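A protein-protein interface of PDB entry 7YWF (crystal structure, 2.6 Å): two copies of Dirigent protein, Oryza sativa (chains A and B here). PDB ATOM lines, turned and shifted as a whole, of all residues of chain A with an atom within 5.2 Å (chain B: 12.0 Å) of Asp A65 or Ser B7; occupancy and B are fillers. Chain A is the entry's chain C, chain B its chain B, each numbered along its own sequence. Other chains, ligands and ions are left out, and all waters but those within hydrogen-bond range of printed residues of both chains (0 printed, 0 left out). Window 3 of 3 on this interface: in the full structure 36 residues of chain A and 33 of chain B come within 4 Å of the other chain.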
ATOM      1  N   THR A  26       0.207   9.381 -25.597  1.00  0.00           N
ATOM      2  CA  THR A  26      -0.606   9.815 -26.720  1.00  0.00           C
ATOM      3  C   THR A  26       0.263   9.809 -27.968  1.00  0.00           C
ATOM      4  O   THR A  26       1.486   9.957 -27.887  1.00  0.00           O
ATOM      5  CB  THR A  26      -1.208  11.211 -26.499  1.00  0.00           C
ATOM      6  OG1 THR A  26      -0.187  12.111 -26.054  1.00  0.00           O
ATOM      7  CG2 THR A  26      -2.322  11.160 -25.462  1.00  0.00           C
ATOM      8  N   LYS A  27      -0.382   9.625 -29.119  1.00  0.00           N
ATOM      9  CA  LYS A  27       0.285   9.679 -30.421  1.00  0.00           C
ATOM     10  C   LYS A  27       1.370   8.609 -30.547  1.00  0.00           C
ATOM     11  O   LYS A  27       2.478   8.873 -31.019  1.00  0.00           O
ATOM     12  CB  LYS A  27       0.863  11.072 -30.690  1.00  0.00           C
ATOM     13  CG  LYS A  27      -0.184  12.168 -30.822  1.00  0.00           C
ATOM     14  N   LEU A  28       1.052   7.391 -30.118  1.00  0.00           N
ATOM     15  CA  LEU A  28       1.857   6.216 -30.423  1.00  0.00           C
ATOM     16  C   LEU A  28       1.245   5.526 -31.633  1.00  0.00           C
ATOM     17  O   LEU A  28       0.025   5.342 -31.692  1.00  0.00           O
ATOM     18  CB  LEU A  28       1.925   5.249 -29.240  1.00  0.00           C
ATOM     19  CG  LEU A  28       2.758   5.655 -28.023  1.00  0.00           C
ATOM     20  CD1 LEU A  28       2.456   4.734 -26.855  1.00  0.00           C
ATOM     21  CD2 LEU A  28       4.241   5.622 -28.355  1.00  0.00           C
ATOM     22  N   TYR A  29       2.085   5.142 -32.590  1.00  0.00           N
ATOM     23  CA  TYR A  29       1.614   4.626 -33.869  1.00  0.00           C
ATOM     24  C   TYR A  29       2.187   3.232 -34.087  1.00  0.00           C
ATOM     25  O   TYR A  29       3.394   3.078 -34.304  1.00  0.00           O
ATOM     26  CB  TYR A  29       2.006   5.575 -35.000  1.00  0.00           C
ATOM     27  CG  TYR A  29       1.395   6.949 -34.844  1.00  0.00           C
ATOM     28  CD1 TYR A  29       0.124   7.228 -35.329  1.00  0.00           C
ATOM     29  CD2 TYR A  29       2.084   7.963 -34.192  1.00  0.00           C
ATOM     30  CE1 TYR A  29      -0.438   8.482 -35.178  1.00  0.00           C
ATOM     31  CE2 TYR A  29       1.531   9.219 -34.037  1.00  0.00           C
ATOM     32  CZ  TYR A  29       0.271   9.473 -34.530  1.00  0.00           C
ATOM     33  OH  TYR A  29      -0.282  10.724 -34.377  1.00  0.00           O
ATOM     34  N   VAL A  63       6.378   0.365 -33.059  1.00  0.00           N
ATOM     35  CA  VAL A  63       5.642   1.520 -32.558  1.00  0.00           C
ATOM     36  C   VAL A  63       6.527   2.749 -32.715  1.00  0.00           C
ATOM     37  O   VAL A  63       7.684   2.746 -32.277  1.00  0.00           O
ATOM     38  CB  VAL A  63       5.216   1.334 -31.089  1.00  0.00           C
ATOM     39  CG1 VAL A  63       4.404   2.529 -30.616  1.00  0.00           C
ATOM     40  CG2 VAL A  63       4.421   0.049 -30.929  1.00  0.00           C
ATOM     41  N   TYR A  64       5.989   3.790 -33.344  1.00  0.00           N
ATOM     42  CA  TYR A  64       6.731   5.011 -33.610  1.00  0.00           C
ATOM     43  C   TYR A  64       6.109   6.192 -32.877  1.00  0.00           C
ATOM     44  O   TYR A  64       4.969   6.134 -32.409  1.00  0.00           O
ATOM     45  CB  TYR A  64       6.786   5.302 -35.116  1.00  0.00           C
ATOM     46  CG  TYR A  64       7.643   4.326 -35.889  1.00  0.00           C
ATOM     47  CD1 TYR A  64       7.141   3.097 -36.291  1.00  0.00           C
ATOM     48  CD2 TYR A  64       8.959   4.633 -36.212  1.00  0.00           C
ATOM     49  CE1 TYR A  64       7.921   2.200 -36.993  1.00  0.00           C
ATOM     50  CE2 TYR A  64       9.747   3.744 -36.915  1.00  0.00           C
ATOM     51  CZ  TYR A  64       9.224   2.529 -37.304  1.00  0.00           C
ATOM     52  OH  TYR A  64      10.006   1.640 -38.004  1.00  0.00           O
ATOM     53  N   ASP A  65       6.882   7.273 -32.785  1.00  0.00           N
ATOM     54  CA  ASP A  65       6.467   8.487 -32.097  1.00  0.00           C
ATOM     55  C   ASP A  65       5.738   9.460 -33.016  1.00  0.00           C
ATOM     56  O   ASP A  65       5.406  10.569 -32.586  1.00  0.00           O
ATOM     57  CB  ASP A  65       7.678   9.180 -31.463  1.00  0.00           C
ATOM     58  CG  ASP A  65       8.763   9.510 -32.472  1.00  0.00           C
ATOM     59  OD1 ASP A  65       8.613   9.153 -33.659  1.00  0.00           O
ATOM     60  OD2 ASP A  65       9.772  10.127 -32.071  1.00  0.00           O
ATOM     61  N   GLY A  66       5.493   9.071 -34.261  1.00  0.00           N
ATOM     62  CA  GLY A  66       4.818   9.937 -35.208  1.00  0.00           C
ATOM     63  C   GLY A  66       4.686   9.234 -36.540  1.00  0.00           C
ATOM     64  O   GLY A  66       5.097   8.081 -36.706  1.00  0.00           O
ATOM     65  N   ILE A  67       4.099   9.949 -37.496  1.00  0.00           N
ATOM     66  CA  ILE A  67       3.838   9.422 -38.829  1.00  0.00           C
ATOM     67  C   ILE A  67       4.753  10.122 -39.825  1.00  0.00           C
ATOM     68  O   ILE A  67       5.035  11.318 -39.693  1.00  0.00           O
ATOM     69  CB  ILE A  67       2.357   9.592 -39.224  1.00  0.00           C
ATOM     70  CG1 ILE A  67       1.934  11.058 -39.116  1.00  0.00           C
ATOM     71  CG2 ILE A  67       1.471   8.711 -38.356  1.00  0.00           C
ATOM     72  CD1 ILE A  67       0.494  11.313 -39.512  1.00  0.00           C
ATOM     73  N   ALA A  71      10.344   9.457 -38.291  1.00  0.00           N
ATOM     74  CA  ALA A  71       9.726   9.151 -37.007  1.00  0.00           C
ATOM     75  C   ALA A  71      10.565   8.126 -36.257  1.00  0.00           C
ATOM     76  O   ALA A  71      10.875   7.054 -36.784  1.00  0.00           O
ATOM     77  CB  ALA A  71       8.304   8.637 -37.218  1.00  0.00           C
ATOM     78  N   LYS A  72      10.945   8.469 -35.030  1.00  0.00           N
ATOM     79  CA  LYS A  72      11.839   7.619 -34.261  1.00  0.00           C
ATOM     80  C   LYS A  72      11.106   6.378 -33.767  1.00  0.00           C
ATOM     81  O   LYS A  72       9.987   6.463 -33.251  1.00  0.00           O
ATOM     82  CB  LYS A  72      12.419   8.396 -33.078  1.00  0.00           C
ATOM     83  CG  LYS A  72      13.364   7.587 -32.203  1.00  0.00           C
ATOM     84  N   LEU A  73      11.737   5.220 -33.939  1.00  0.00           N
ATOM     85  CA  LEU A  73      11.224   3.986 -33.359  1.00  0.00           C
ATOM     86  C   LEU A  73      11.306   4.072 -31.842  1.00  0.00           C
ATOM     87  O   LEU A  73      12.381   4.316 -31.285  1.00  0.00           O
ATOM     88  CB  LEU A  73      12.025   2.795 -33.872  1.00  0.00           C
ATOM     89  CG  LEU A  73      11.642   1.422 -33.326  1.00  0.00           C
ATOM     90  CD1 LEU A  73      10.344   0.929 -33.945  1.00  0.00           C
ATOM     91  CD2 LEU A  73      12.771   0.437 -33.564  1.00  0.00           C
ATOM     92  N   VAL A  74      10.176   3.871 -31.169  1.00  0.00           N
ATOM     93  CA  VAL A  74      10.133   3.997 -29.720  1.00  0.00           C
ATOM     94  C   VAL A  74       9.786   2.696 -29.014  1.00  0.00           C
ATOM     95  O   VAL A  74      10.147   2.540 -27.837  1.00  0.00           O
ATOM     96  CB  VAL A  74       9.155   5.109 -29.284  1.00  0.00           C
ATOM     97  CG1 VAL A  74       9.631   6.463 -29.790  1.00  0.00           C
ATOM     98  CG2 VAL A  74       7.746   4.805 -29.770  1.00  0.00           C
ATOM     99  N   SER B   7       5.583  11.266 -29.978  1.00  0.00           N
ATOM    100  CA  SER B   7       4.629  10.865 -28.951  1.00  0.00           C
ATOM    101  C   SER B   7       4.727  11.773 -27.729  1.00  0.00           C
ATOM    102  O   SER B   7       5.603  12.634 -27.651  1.00  0.00           O
ATOM    103  CB  SER B   7       4.854   9.406 -28.548  1.00  0.00           C
ATOM    104  OG  SER B   7       6.165   9.215 -28.049  1.00  0.00           O
ATOM    105  N   LYS B   8       3.830  11.563 -26.769  1.00  0.00           N
ATOM    106  CA  LYS B   8       3.745  12.399 -25.580  1.00  0.00           C
ATOM    107  C   LYS B   8       3.387  11.530 -24.387  1.00  0.00           C
ATOM    108  O   LYS B   8       2.395  10.798 -24.425  1.00  0.00           O
ATOM    109  CB  LYS B   8       2.701  13.506 -25.758  1.00  0.00           C
ATOM    110  CG  LYS B   8       2.455  14.336 -24.512  1.00  0.00           C
ATOM    111  CD  LYS B   8       1.351  15.350 -24.747  1.00  0.00           C
ATOM    112  CE  LYS B   8       1.033  16.115 -23.480  1.00  0.00           C
ATOM    113  NZ  LYS B   8      -0.081  17.082 -23.676  1.00  0.00           N
ATOM    114  N   LEU B   9       4.186  11.628 -23.328  1.00  0.00           N
ATOM    115  CA  LEU B   9       3.990  10.854 -22.108  1.00  0.00           C
ATOM    116  C   LEU B   9       3.787  11.808 -20.940  1.00  0.00           C
ATOM    117  O   LEU B   9       4.701  12.554 -20.580  1.00  0.00           O
ATOM    118  CB  LEU B   9       5.180   9.927 -21.850  1.00  0.00           C
ATOM    119  CG  LEU B   9       5.278   9.319 -20.450  1.00  0.00           C
ATOM    120  CD1 LEU B   9       4.071   8.448 -20.140  1.00  0.00           C
ATOM    121  CD2 LEU B   9       6.567   8.523 -20.306  1.00  0.00           C
ATOM    122  N   GLN B  10       2.597  11.774 -20.350  1.00  0.00           N
ATOM    123  CA  GLN B  10       2.282  12.579 -19.181  1.00  0.00           C
ATOM    124  C   GLN B  10       2.295  11.707 -17.935  1.00  0.00           C
ATOM    125  O   GLN B  10       1.754  10.597 -17.934  1.00  0.00           O
ATOM    126  CB  GLN B  10       0.907  13.237 -19.324  1.00  0.00           C
ATOM    127  CG  GLN B  10       0.856  14.412 -20.278  1.00  0.00           C
ATOM    128  CD  GLN B  10      -0.465  15.153 -20.199  1.00  0.00           C
ATOM    129  OE1 GLN B  10      -1.523  14.587 -20.476  1.00  0.00           O
ATOM    130  NE2 GLN B  10      -0.410  16.425 -19.820  1.00  0.00           N
ATOM    131  N   ILE B  11       2.910  12.216 -16.873  1.00  0.00           N
ATOM    132  CA  ILE B  11       2.996  11.518 -15.596  1.00  0.00           C
ATOM    133  C   ILE B  11       2.387  12.417 -14.532  1.00  0.00           C
ATOM    134  O   ILE B  11       2.844  13.549 -14.332  1.00  0.00           O
ATOM    135  CB  ILE B  11       4.444  11.142 -15.243  1.00  0.00           C
ATOM    136  CG1 ILE B  11       5.083  10.352 -16.387  1.00  0.00           C
ATOM    137  CG2 ILE B  11       4.485  10.342 -13.956  1.00  0.00           C
ATOM    138  CD1 ILE B  11       6.519   9.955 -16.130  1.00  0.00           C
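Thr A26 touches two residues of chain B.
Leu A28 touches just one residue of chain B: Ser B7 (3.8 Å).
No residue of chain B comes within 4 Å of Tyr A29.
No residue of chain B comes within 4 Å of Val A63.
Of chain B, only Ser B7 (2.7 Å) comes within 4 Å of Asp A65.
No residue of chain B comes within 4 Å of Ala A71.
Ser B7 touches just these residues of chain A: Thr A26 (3.4 Å), Lys A27 (3.5 Å), Leu A28 (3.8 Å) and Asp A65 (2.7 Å).
Printed residues of chain A within 4 Å of Lys B8: Thr A26.
The nearest residue of chain B that does not touch Asp A65 is Lys B8 (6.1 Å).
The nearest residue of chain A that does not touch Ser B7 is Val A74 (4.8 Å).
The side-chain carboxylate of Asp A65 is in hydrogen-bond range of the backbone NH of Lys A72, at 2.8 Å.
No position is printed for both chains.
Of the 5 pairs that touch across the chains among the printed residues, none has its exchanged pair printed and touching as well.
Along chain B the printed residues that touch a printed residue of chain A span positions 7 to 8.
Of the 13 printed residues of chain A, 4 touch a printed residue of chain B.
Printed residues of chain A that touch a printed residue of chain B: Thr A26, Lys A27, Leu A28 and Asp A65.
Hydrophobic or aromatic side chains of chain A that line the printed part of chain B: Leu A28.
Along chain A the printed residues that touch a printed residue of chain B span positions 26 to 65.
Among the printed residues, no Asp or Glu carboxylate lies within 4 Å of a Lys or Arg side-chain nitrogen of the other chain.
The backbone carbonyl oxygen of Asp A65 lies within hydrogen-bond range of the backbone NH of Ser B7 (2.7 Å).
N of Thr A26 sits at hydrogen-bond distance from O of Lys B8, at 2.9 Å.
Among the printed residues, merely in contact across the chains: Thr A26 with Ser B7, Lys A27 with Ser B7 and Leu A28 with Ser B7.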
